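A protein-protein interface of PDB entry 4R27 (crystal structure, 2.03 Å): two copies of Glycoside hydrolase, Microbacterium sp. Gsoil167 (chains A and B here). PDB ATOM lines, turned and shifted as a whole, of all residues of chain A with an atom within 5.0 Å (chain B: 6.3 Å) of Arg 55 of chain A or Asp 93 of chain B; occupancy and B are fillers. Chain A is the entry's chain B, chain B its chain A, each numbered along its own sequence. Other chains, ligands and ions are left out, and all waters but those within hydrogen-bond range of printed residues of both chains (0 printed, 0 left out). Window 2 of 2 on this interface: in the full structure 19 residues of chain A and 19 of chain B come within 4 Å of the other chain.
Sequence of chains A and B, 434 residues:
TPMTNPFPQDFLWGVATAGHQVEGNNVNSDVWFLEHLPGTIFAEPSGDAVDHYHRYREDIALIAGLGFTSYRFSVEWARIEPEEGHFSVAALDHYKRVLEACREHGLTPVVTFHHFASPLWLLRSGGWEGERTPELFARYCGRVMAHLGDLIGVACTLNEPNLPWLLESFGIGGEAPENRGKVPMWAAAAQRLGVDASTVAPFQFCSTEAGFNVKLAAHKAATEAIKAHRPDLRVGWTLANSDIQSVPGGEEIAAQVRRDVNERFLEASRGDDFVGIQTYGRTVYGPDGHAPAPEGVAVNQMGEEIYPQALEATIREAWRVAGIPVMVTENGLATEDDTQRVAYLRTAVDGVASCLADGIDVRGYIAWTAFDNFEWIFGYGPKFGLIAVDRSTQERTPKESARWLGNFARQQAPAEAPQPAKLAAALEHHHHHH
Arg 55 of chain A touches one residue of chain B.
Asp 93 of chain B touches one residue of chain A.
Of the printed residues of chain A, Ala 90 of chain B touches Asp 51.
Of the printed residues of chain B, His 54 of chain A touches Arg 97.
Of the printed residues of chain A, Arg 97 of chain B touches His 54.
Glu 100 of chain B touches none of the printed residues of chain A.
Arg 57 of chain A touches none of the printed residues of chain B.
Of the 13 printed residues of chain A, 3 touch a printed residue of chain B.
Hydrophobic or aromatic side chains of chain A within 4 Å of the printed part of chain B: His 54.
Of the 15 printed residues of chain B, 3 touch a printed residue of chain A.
Hydrophobic or aromatic side chains of chain B that line the printed part of chain A: Ala 90.
Among the printed residues, 3 pairs touch across the chains.
The side-chain carboxylate of Asp 93 of chain B lies within hydrogen-bond range of a ring nitrogen (NE2) of His 147 of chain B.
The guanidinium group of Arg 55 of chain A lies within salt-bridge range of the side-chain carboxylate of Asp 51 of chain A (3.4 Å).
OG of Ser 88 of chain B sits close to N of Ala 90 of chain B, at 3.4 Å.
The side-chain carboxylate (OD1) of Asp 51 of chain A is in hydrogen-bond range of a ring nitrogen (ND1) of His 54 of chain A (2.6 Å).
O of Asp 93 of chain B lies close to NH1 of Arg 97 of chain B (3.5 Å).
1 position is printed for both chains.
Of the 3 pairs that touch across the chains among the printed residues, none has its exchanged pair printed and touching as well.
The side-chain carboxylate (OD2) of Asp 93 of chain B lies within salt-bridge range of the guanidinium group (NH2) of Arg 55 of chain A (3.7 Å).
OD1 of Asp 51 of chain A touches CB of Ala 90 of chain B, 3.5 Å away.
His 54 of chain A touches Arg 97 of chain B.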
ATOM      1  N   VAL A  50       7.356  -5.695 -10.816  1.00  0.00           N
ATOM      2  CA  VAL A  50       8.764  -5.324 -10.722  1.00  0.00           C
ATOM      3  C   VAL A  50       9.357  -5.031 -12.092  1.00  0.00           C
ATOM      4  O   VAL A  50      10.589  -5.077 -12.256  1.00  0.00           O
ATOM      5  CB  VAL A  50       9.639  -6.383  -9.965  1.00  0.00           C
ATOM      6  CG1 VAL A  50       9.158  -6.543  -8.539  1.00  0.00           C
ATOM      7  CG2 VAL A  50       9.743  -7.744 -10.699  1.00  0.00           C
ATOM      8  N   ASP A  51       8.491  -4.725 -13.070  1.00  0.00           N
ATOM      9  CA  ASP A  51       8.900  -4.416 -14.430  1.00  0.00           C
ATOM     10  C   ASP A  51       9.924  -5.392 -15.049  1.00  0.00           C
ATOM     11  O   ASP A  51      10.845  -4.984 -15.758  1.00  0.00           O
ATOM     12  CB  ASP A  51       9.378  -2.993 -14.458  1.00  0.00           C
ATOM     13  CG  ASP A  51       9.545  -2.458 -15.834  1.00  0.00           C
ATOM     14  OD1 ASP A  51       8.915  -2.985 -16.796  1.00  0.00           O
ATOM     15  OD2 ASP A  51      10.376  -1.514 -15.973  1.00  0.00           O
ATOM     16  N   HIS A  52       9.739  -6.688 -14.782  1.00  0.00           N
ATOM     17  CA  HIS A  52      10.550  -7.739 -15.388  1.00  0.00           C
ATOM     18  C   HIS A  52      10.471  -7.762 -16.923  1.00  0.00           C
ATOM     19  O   HIS A  52      11.436  -8.165 -17.562  1.00  0.00           O
ATOM     20  CB  HIS A  52      10.187  -9.131 -14.783  1.00  0.00           C
ATOM     21  CG  HIS A  52      11.037 -10.244 -15.281  1.00  0.00           C
ATOM     22  ND1 HIS A  52      12.410 -10.261 -15.116  1.00  0.00           N
ATOM     23  CD2 HIS A  52      10.720 -11.393 -15.930  1.00  0.00           C
ATOM     24  CE1 HIS A  52      12.884 -11.394 -15.601  1.00  0.00           C
ATOM     25  NE2 HIS A  52      11.884 -12.085 -16.120  1.00  0.00           N
ATOM     26  N   TYR A  53       9.352  -7.317 -17.505  1.00  0.00           N
ATOM     27  CA  TYR A  53       9.204  -7.215 -18.947  1.00  0.00           C
ATOM     28  C   TYR A  53      10.358  -6.394 -19.521  1.00  0.00           C
ATOM     29  O   TYR A  53      10.940  -6.747 -20.555  1.00  0.00           O
ATOM     30  CB  TYR A  53       7.832  -6.533 -19.343  1.00  0.00           C
ATOM     31  CG  TYR A  53       7.538  -6.613 -20.815  1.00  0.00           C
ATOM     32  CD1 TYR A  53       6.728  -7.592 -21.324  1.00  0.00           C
ATOM     33  CD2 TYR A  53       8.149  -5.762 -21.696  1.00  0.00           C
ATOM     34  CE1 TYR A  53       6.531  -7.717 -22.688  1.00  0.00           C
ATOM     35  CE2 TYR A  53       7.924  -5.818 -23.049  1.00  0.00           C
ATOM     36  CZ  TYR A  53       7.114  -6.803 -23.553  1.00  0.00           C
ATOM     37  OH  TYR A  53       6.968  -6.857 -24.912  1.00  0.00           O
ATOM     38  N   HIS A  54      10.692  -5.280 -18.865  1.00  0.00           N
ATOM     39  CA  HIS A  54      11.784  -4.451 -19.396  1.00  0.00           C
ATOM     40  C   HIS A  54      13.170  -4.763 -18.884  1.00  0.00           C
ATOM     41  O   HIS A  54      14.135  -4.434 -19.558  1.00  0.00           O
ATOM     42  CB  HIS A  54      11.501  -2.948 -19.263  1.00  0.00           C
ATOM     43  CG  HIS A  54      10.264  -2.516 -19.961  1.00  0.00           C
ATOM     44  ND1 HIS A  54       9.068  -2.343 -19.304  1.00  0.00           N
ATOM     45  CD2 HIS A  54      10.035  -2.198 -21.255  1.00  0.00           C
ATOM     46  CE1 HIS A  54       8.138  -1.972 -20.165  1.00  0.00           C
ATOM     47  NE2 HIS A  54       8.705  -1.881 -21.357  1.00  0.00           N
ATOM     48  N   ARG A  55      13.272  -5.366 -17.707  1.00  0.00           N
ATOM     49  CA  ARG A  55      14.560  -5.515 -17.024  1.00  0.00           C
ATOM     50  C   ARG A  55      15.043  -6.938 -17.105  1.00  0.00           C
ATOM     51  O   ARG A  55      15.977  -7.318 -16.400  1.00  0.00           O
ATOM     52  CB  ARG A  55      14.413  -5.136 -15.526  1.00  0.00           C
ATOM     53  CG  ARG A  55      14.203  -3.688 -15.383  1.00  0.00           C
ATOM     54  CD  ARG A  55      13.646  -3.243 -14.058  1.00  0.00           C
ATOM     55  NE  ARG A  55      13.307  -1.816 -14.233  1.00  0.00           N
ATOM     56  CZ  ARG A  55      14.067  -0.798 -13.846  1.00  0.00           C
ATOM     57  NH1 ARG A  55      15.211  -0.991 -13.208  1.00  0.00           N
ATOM     58  NH2 ARG A  55      13.631   0.414 -14.052  1.00  0.00           N
ATOM     59  N   TYR A  56      14.431  -7.771 -17.924  1.00  0.00           N
ATOM     60  CA  TYR A  56      14.759  -9.195 -17.835  1.00  0.00           C
ATOM     61  C   TYR A  56      16.249  -9.521 -18.010  1.00  0.00           C
ATOM     62  O   TYR A  56      16.770 -10.502 -17.439  1.00  0.00           O
ATOM     63  CB  TYR A  56      13.933 -10.002 -18.824  1.00  0.00           C
ATOM     64  CG  TYR A  56      14.123  -9.622 -20.296  1.00  0.00           C
ATOM     65  CD1 TYR A  56      15.080 -10.255 -21.073  1.00  0.00           C
ATOM     66  CD2 TYR A  56      13.358  -8.615 -20.877  1.00  0.00           C
ATOM     67  CE1 TYR A  56      15.258  -9.935 -22.400  1.00  0.00           C
ATOM     68  CE2 TYR A  56      13.535  -8.255 -22.210  1.00  0.00           C
ATOM     69  CZ  TYR A  56      14.470  -8.937 -22.964  1.00  0.00           C
ATOM     70  OH  TYR A  56      14.633  -8.674 -24.275  1.00  0.00           O
ATOM     71  N   ARG A  57      16.945  -8.730 -18.801  1.00  0.00           N
ATOM     72  CA  ARG A  57      18.322  -9.063 -19.093  1.00  0.00           C
ATOM     73  C   ARG A  57      19.164  -8.961 -17.859  1.00  0.00           C
ATOM     74  O   ARG A  57      20.012  -9.798 -17.623  1.00  0.00           O
ATOM     75  CB  ARG A  57      18.891  -8.166 -20.227  1.00  0.00           C
ATOM     76  CG  ARG A  57      18.574  -8.757 -21.580  1.00  0.00           C
ATOM     77  CD  ARG A  57      19.352  -8.136 -22.732  1.00  0.00           C
ATOM     78  NE  ARG A  57      20.807  -8.245 -22.569  1.00  0.00           N
ATOM     79  CZ  ARG A  57      21.541  -9.345 -22.744  1.00  0.00           C
ATOM     80  NH1 ARG A  57      20.977 -10.515 -23.053  1.00  0.00           N
ATOM     81  NH2 ARG A  57      22.861  -9.266 -22.608  1.00  0.00           N
ATOM     82  N   GLU A  58      18.949  -7.880 -17.125  1.00  0.00           N
ATOM     83  CA  GLU A  58      19.652  -7.577 -15.909  1.00  0.00           C
ATOM     84  C   GLU A  58      19.228  -8.621 -14.860  1.00  0.00           C
ATOM     85  O   GLU A  58      20.097  -9.154 -14.104  1.00  0.00           O
ATOM     86  CB  GLU A  58      19.352  -6.123 -15.486  1.00  0.00           C
ATOM     87  CG  GLU A  58      19.948  -5.069 -16.436  1.00  0.00           C
ATOM     88  CD  GLU A  58      19.326  -5.012 -17.850  1.00  0.00           C
ATOM     89  OE1 GLU A  58      18.077  -5.093 -17.994  1.00  0.00           O
ATOM     90  OE2 GLU A  58      20.117  -4.902 -18.852  1.00  0.00           O
ATOM     91  N   ASP A  59      17.923  -8.969 -14.837  1.00  0.00           N
ATOM     92  CA  ASP A  59      17.435  -9.949 -13.906  1.00  0.00           C
ATOM     93  C   ASP A  59      18.080 -11.344 -14.064  1.00  0.00           C
ATOM     94  O   ASP A  59      18.409 -12.006 -13.036  1.00  0.00           O
ATOM     95  CB  ASP A  59      15.933 -10.087 -14.005  1.00  0.00           C
ATOM     96  CG  ASP A  59      15.232  -8.932 -13.408  1.00  0.00           C
ATOM     97  OD1 ASP A  59      15.920  -8.135 -12.727  1.00  0.00           O
ATOM     98  OD2 ASP A  59      14.007  -8.804 -13.614  1.00  0.00           O
ATOM     99  N   THR A 393      11.866   2.399  -6.982  1.00  0.00           N
ATOM    100  CA  THR A 393      13.016   2.560  -7.928  1.00  0.00           C
ATOM    101  C   THR A 393      13.306   1.378  -8.872  1.00  0.00           C
ATOM    102  O   THR A 393      14.143   1.511  -9.792  1.00  0.00           O
ATOM    103  CB  THR A 393      14.343   2.720  -7.180  1.00  0.00           C
ATOM    104  OG1 THR A 393      14.518   1.578  -6.354  1.00  0.00           O
ATOM    105  CG2 THR A 393      14.347   3.973  -6.251  1.00  0.00           C
ATOM    106  N   GLN A 394      12.652   0.230  -8.597  1.00  0.00           N
ATOM    107  CA  GLN A 394      12.859  -1.065  -9.265  1.00  0.00           C
ATOM    108  C   GLN A 394      14.249  -1.674  -8.980  1.00  0.00           C
ATOM    109  O   GLN A 394      14.685  -2.631  -9.635  1.00  0.00           O
ATOM    110  CB  GLN A 394      12.474  -0.980 -10.763  1.00  0.00           C
ATOM    111  CG  GLN A 394      10.963  -0.681 -11.011  1.00  0.00           C
ATOM    112  CD  GLN A 394      10.035  -1.854 -10.622  1.00  0.00           C
ATOM    113  OE1 GLN A 394      10.457  -2.805  -9.956  1.00  0.00           O
ATOM    114  NE2 GLN A 394       8.747  -1.780 -11.024  1.00  0.00           N
ATOM    115  N   ARG A 396      17.030  -3.904  -7.521  1.00  0.00           N
ATOM    116  CA  ARG A 396      17.074  -5.289  -7.008  1.00  0.00           C
ATOM    117  C   ARG A 396      18.141  -5.441  -5.872  1.00  0.00           C
ATOM    118  O   ARG A 396      19.294  -5.075  -6.061  1.00  0.00           O
ATOM    119  CB  ARG A 396      17.471  -6.287  -8.106  1.00  0.00           C
ATOM    120  CG  ARG A 396      16.375  -6.773  -9.046  1.00  0.00           C
ATOM    121  CD  ARG A 396      15.712  -5.642  -9.799  1.00  0.00           C
ATOM    122  NE  ARG A 396      14.834  -6.176 -10.809  1.00  0.00           N
ATOM    123  CZ  ARG A 396      13.615  -5.754 -11.107  1.00  0.00           C
ATOM    124  NH1 ARG A 396      13.072  -4.732 -10.464  1.00  0.00           N
ATOM    125  NH2 ARG A 396      12.970  -6.326 -12.146  1.00  0.00           N
ATOM    126  N   TYR B  56      12.781   0.692 -31.496  1.00  0.00           N
ATOM    127  CA  TYR B  56      12.950   2.154 -31.650  1.00  0.00           C
ATOM    128  C   TYR B  56      14.428   2.540 -31.731  1.00  0.00           C
ATOM    129  O   TYR B  56      14.808   3.425 -32.477  1.00  0.00           O
ATOM    130  CB  TYR B  56      12.233   2.857 -30.506  1.00  0.00           C
ATOM    131  CG  TYR B  56      12.772   2.507 -29.158  1.00  0.00           C
ATOM    132  CD1 TYR B  56      13.799   3.260 -28.571  1.00  0.00           C
ATOM    133  CD2 TYR B  56      12.214   1.471 -28.412  1.00  0.00           C
ATOM    134  CE1 TYR B  56      14.303   2.953 -27.298  1.00  0.00           C
ATOM    135  CE2 TYR B  56      12.697   1.154 -27.128  1.00  0.00           C
ATOM    136  CZ  TYR B  56      13.756   1.871 -26.599  1.00  0.00           C
ATOM    137  OH  TYR B  56      14.210   1.565 -25.361  1.00  0.00           O
ATOM    138  N   SER B  88       1.805   4.300 -14.965  1.00  0.00           N
ATOM    139  CA  SER B  88       2.826   3.296 -15.132  1.00  0.00           C
ATOM    140  C   SER B  88       4.176   3.913 -15.286  1.00  0.00           C
ATOM    141  O   SER B  88       4.503   4.455 -16.335  1.00  0.00           O
ATOM    142  CB  SER B  88       2.524   2.349 -16.318  1.00  0.00           C
ATOM    143  OG  SER B  88       3.642   1.500 -16.588  1.00  0.00           O
ATOM    144  N   VAL B  89       4.997   3.764 -14.242  1.00  0.00           N
ATOM    145  CA  VAL B  89       6.373   4.252 -14.280  1.00  0.00           C
ATOM    146  C   VAL B  89       7.165   3.384 -15.315  1.00  0.00           C
ATOM    147  O   VAL B  89       8.087   3.876 -15.987  1.00  0.00           O
ATOM    148  CB  VAL B  89       7.024   4.206 -12.862  1.00  0.00           C
ATOM    149  CG1 VAL B  89       8.520   4.444 -12.949  1.00  0.00           C
ATOM    150  CG2 VAL B  89       6.379   5.247 -11.876  1.00  0.00           C
ATOM    151  N   ALA B  90       6.825   2.099 -15.412  1.00  0.00           N
ATOM    152  CA  ALA B  90       7.419   1.205 -16.405  1.00  0.00           C
ATOM    153  C   ALA B  90       7.210   1.758 -17.834  1.00  0.00           C
ATOM    154  O   ALA B  90       8.106   1.751 -18.648  1.00  0.00           O
ATOM    155  CB  ALA B  90       6.782  -0.203 -16.299  1.00  0.00           C
ATOM    156  N   ALA B  91       6.022   2.197 -18.166  1.00  0.00           N
ATOM    157  CA  ALA B  91       5.811   2.741 -19.531  1.00  0.00           C
ATOM    158  C   ALA B  91       6.504   4.098 -19.669  1.00  0.00           C
ATOM    159  O   ALA B  91       7.046   4.401 -20.713  1.00  0.00           O
ATOM    160  CB  ALA B  91       4.379   2.924 -19.827  1.00  0.00           C
ATOM    161  N   LEU B  92       6.479   4.894 -18.624  1.00  0.00           N
ATOM    162  CA  LEU B  92       7.142   6.231 -18.679  1.00  0.00           C
ATOM    163  C   LEU B  92       8.667   6.020 -18.909  1.00  0.00           C
ATOM    164  O   LEU B  92       9.300   6.759 -19.671  1.00  0.00           O
ATOM    165  CB  LEU B  92       6.836   7.088 -17.406  1.00  0.00           C
ATOM    166  CG  LEU B  92       5.477   7.829 -17.301  1.00  0.00           C
ATOM    167  CD1 LEU B  92       5.105   8.228 -15.886  1.00  0.00           C
ATOM    168  CD2 LEU B  92       5.509   9.099 -18.150  1.00  0.00           C
ATOM    169  N   ASP B  93       9.248   5.006 -18.287  1.00  0.00           N
ATOM    170  CA  ASP B  93      10.674   4.656 -18.496  1.00  0.00           C
ATOM    171  C   ASP B  93      10.945   4.185 -19.939  1.00  0.00           C
ATOM    172  O   ASP B  93      12.031   4.386 -20.464  1.00  0.00           O
ATOM    173  CB  ASP B  93      11.115   3.548 -17.538  1.00  0.00           C
ATOM    174  CG  ASP B  93      11.669   4.073 -16.253  1.00  0.00           C
ATOM    175  OD1 ASP B  93      12.248   5.186 -16.265  1.00  0.00           O
ATOM    176  OD2 ASP B  93      11.583   3.331 -15.215  1.00  0.00           O
ATOM    177  N   HIS B  94       9.952   3.546 -20.559  1.00  0.00           N
ATOM    178  CA  HIS B  94      10.087   3.146 -21.941  1.00  0.00           C
ATOM    179  C   HIS B  94      10.301   4.387 -22.793  1.00  0.00           C
ATOM    180  O   HIS B  94      11.237   4.459 -23.615  1.00  0.00           O
ATOM    181  CB  HIS B  94       8.924   2.289 -22.393  1.00  0.00           C
ATOM    182  CG  HIS B  94       8.857   2.175 -23.864  1.00  0.00           C
ATOM    183  ND1 HIS B  94       8.043   2.978 -24.625  1.00  0.00           N
ATOM    184  CD2 HIS B  94       9.617   1.478 -24.732  1.00  0.00           C
ATOM    185  CE1 HIS B  94       8.249   2.724 -25.912  1.00  0.00           C
ATOM    186  NE2 HIS B  94       9.206   1.827 -25.997  1.00  0.00           N
ATOM    187  N   TYR B  95       9.477   5.392 -22.561  1.00  0.00           N
ATOM    188  CA  TYR B  95       9.539   6.584 -23.399  1.00  0.00           C
ATOM    189  C   TYR B  95      10.726   7.435 -23.034  1.00  0.00           C
ATOM    190  O   TYR B  95      11.255   8.146 -23.866  1.00  0.00           O
ATOM    191  CB  TYR B  95       8.253   7.366 -23.304  1.00  0.00           C
ATOM    192  CG  TYR B  95       7.130   6.683 -24.026  1.00  0.00           C
ATOM    193  CD1 TYR B  95       7.111   6.685 -25.400  1.00  0.00           C
ATOM    194  CD2 TYR B  95       6.072   6.043 -23.334  1.00  0.00           C
ATOM    195  CE1 TYR B  95       6.067   6.097 -26.091  1.00  0.00           C
ATOM    196  CE2 TYR B  95       5.029   5.462 -24.021  1.00  0.00           C
ATOM    197  CZ  TYR B  95       5.041   5.549 -25.424  1.00  0.00           C
ATOM    198  OH  TYR B  95       4.087   5.029 -26.218  1.00  0.00           O
ATOM    199  N   LYS B  96      11.213   7.308 -21.807  1.00  0.00           N
ATOM    200  CA  LYS B  96      12.471   7.980 -21.476  1.00  0.00           C
ATOM    201  C   LYS B  96      13.694   7.386 -22.248  1.00  0.00           C
ATOM    202  O   LYS B  96      14.505   8.111 -22.809  1.00  0.00           O
ATOM    203  CB  LYS B  96      12.661   7.885 -19.988  1.00  0.00           C
ATOM    204  CG  LYS B  96      13.642   8.858 -19.397  1.00  0.00           C
ATOM    205  CD  LYS B  96      13.910   8.340 -18.002  1.00  0.00           C
ATOM    206  CE  LYS B  96      15.236   8.855 -17.473  1.00  0.00           C
ATOM    207  NZ  LYS B  96      14.984  10.199 -16.901  1.00  0.00           N
ATOM    208  N   ARG B  97      13.786   6.065 -22.337  1.00  0.00           N
ATOM    209  CA  ARG B  97      14.758   5.411 -23.208  1.00  0.00           C
ATOM    210  C   ARG B  97      14.618   5.763 -24.691  1.00  0.00           C
ATOM    211  O   ARG B  97      15.622   5.858 -25.419  1.00  0.00           O
ATOM    212  CB  ARG B  97      14.732   3.893 -22.989  1.00  0.00           C
ATOM    213  CG  ARG B  97      15.208   3.509 -21.580  1.00  0.00           C
ATOM    214  CD  ARG B  97      15.337   1.997 -21.427  1.00  0.00           C
ATOM    215  NE  ARG B  97      14.074   1.267 -21.433  1.00  0.00           N
ATOM    216  CZ  ARG B  97      13.303   1.069 -20.369  1.00  0.00           C
ATOM    217  NH1 ARG B  97      13.627   1.564 -19.170  1.00  0.00           N
ATOM    218  NH2 ARG B  97      12.178   0.401 -20.494  1.00  0.00           N
ATOM    219  N   VAL B  98      13.399   5.978 -25.160  1.00  0.00           N
ATOM    220  CA  VAL B  98      13.195   6.476 -26.523  1.00  0.00           C
ATOM    221  C   VAL B  98      13.822   7.860 -26.657  1.00  0.00           C
ATOM    222  O   VAL B  98      14.621   8.100 -27.558  1.00  0.00           O
ATOM    223  CB  VAL B  98      11.707   6.459 -26.939  1.00  0.00           C
ATOM    224  CG1 VAL B  98      11.465   7.081 -28.274  1.00  0.00           C
ATOM    225  CG2 VAL B  98      11.130   5.029 -26.936  1.00  0.00           C
ATOM    226  N   GLU B 100      16.161   9.269 -24.780  1.00  0.00           N
ATOM    227  CA  GLU B 100      17.583   9.041 -24.648  1.00  0.00           C
ATOM    228  C   GLU B 100      18.223   8.520 -25.921  1.00  0.00           C
ATOM    229  O   GLU B 100      19.329   8.918 -26.280  1.00  0.00           O
ATOM    230  CB  GLU B 100      17.802   8.011 -23.529  1.00  0.00           C
ATOM    231  CG  GLU B 100      17.571   8.641 -22.159  1.00  0.00           C
ATOM    232  CD  GLU B 100      17.692   7.665 -21.001  1.00  0.00           C
ATOM    233  OE1 GLU B 100      17.905   6.467 -21.233  1.00  0.00           O
ATOM    234  OE2 GLU B 100      17.600   8.160 -19.845  1.00  0.00           O
ATOM    235  N   HIS B 147       8.663  12.769 -15.236  1.00  0.00           N
ATOM    236  CA  HIS B 147       9.580  11.670 -15.411  1.00  0.00           C
ATOM    237  C   HIS B 147      10.588  11.931 -16.520  1.00  0.00           C
ATOM    238  O   HIS B 147      11.685  11.511 -16.418  1.00  0.00           O
ATOM    239  CB  HIS B 147       8.748  10.413 -15.700  1.00  0.00           C
ATOM    240  CG  HIS B 147       9.538   9.152 -15.643  1.00  0.00           C
ATOM    241  ND1 HIS B 147       9.667   8.410 -14.490  1.00  0.00           N
ATOM    242  CD2 HIS B 147      10.269   8.520 -16.579  1.00  0.00           C
ATOM    243  CE1 HIS B 147      10.417   7.347 -14.732  1.00  0.00           C
ATOM    244  NE2 HIS B 147      10.833   7.412 -15.982  1.00  0.00           N
ATOM    245  N   LEU B 148      10.258  12.644 -17.597  1.00  0.00           N
ATOM    246  CA  LEU B 148      11.224  12.714 -18.726  1.00  0.00           C
ATOM    247  C   LEU B 148      11.229  14.070 -19.453  1.00  0.00           C
ATOM    248  O   LEU B 148      11.847  14.236 -20.509  1.00  0.00           O
ATOM    249  CB  LEU B 148      10.987  11.537 -19.700  1.00  0.00           C
ATOM    250  CG  LEU B 148       9.537  11.382 -20.177  1.00  0.00           C
ATOM    251  CD1 LEU B 148       9.171  12.622 -20.997  1.00  0.00           C
ATOM    252  CD2 LEU B 148       9.272  10.072 -20.965  1.00  0.00           C
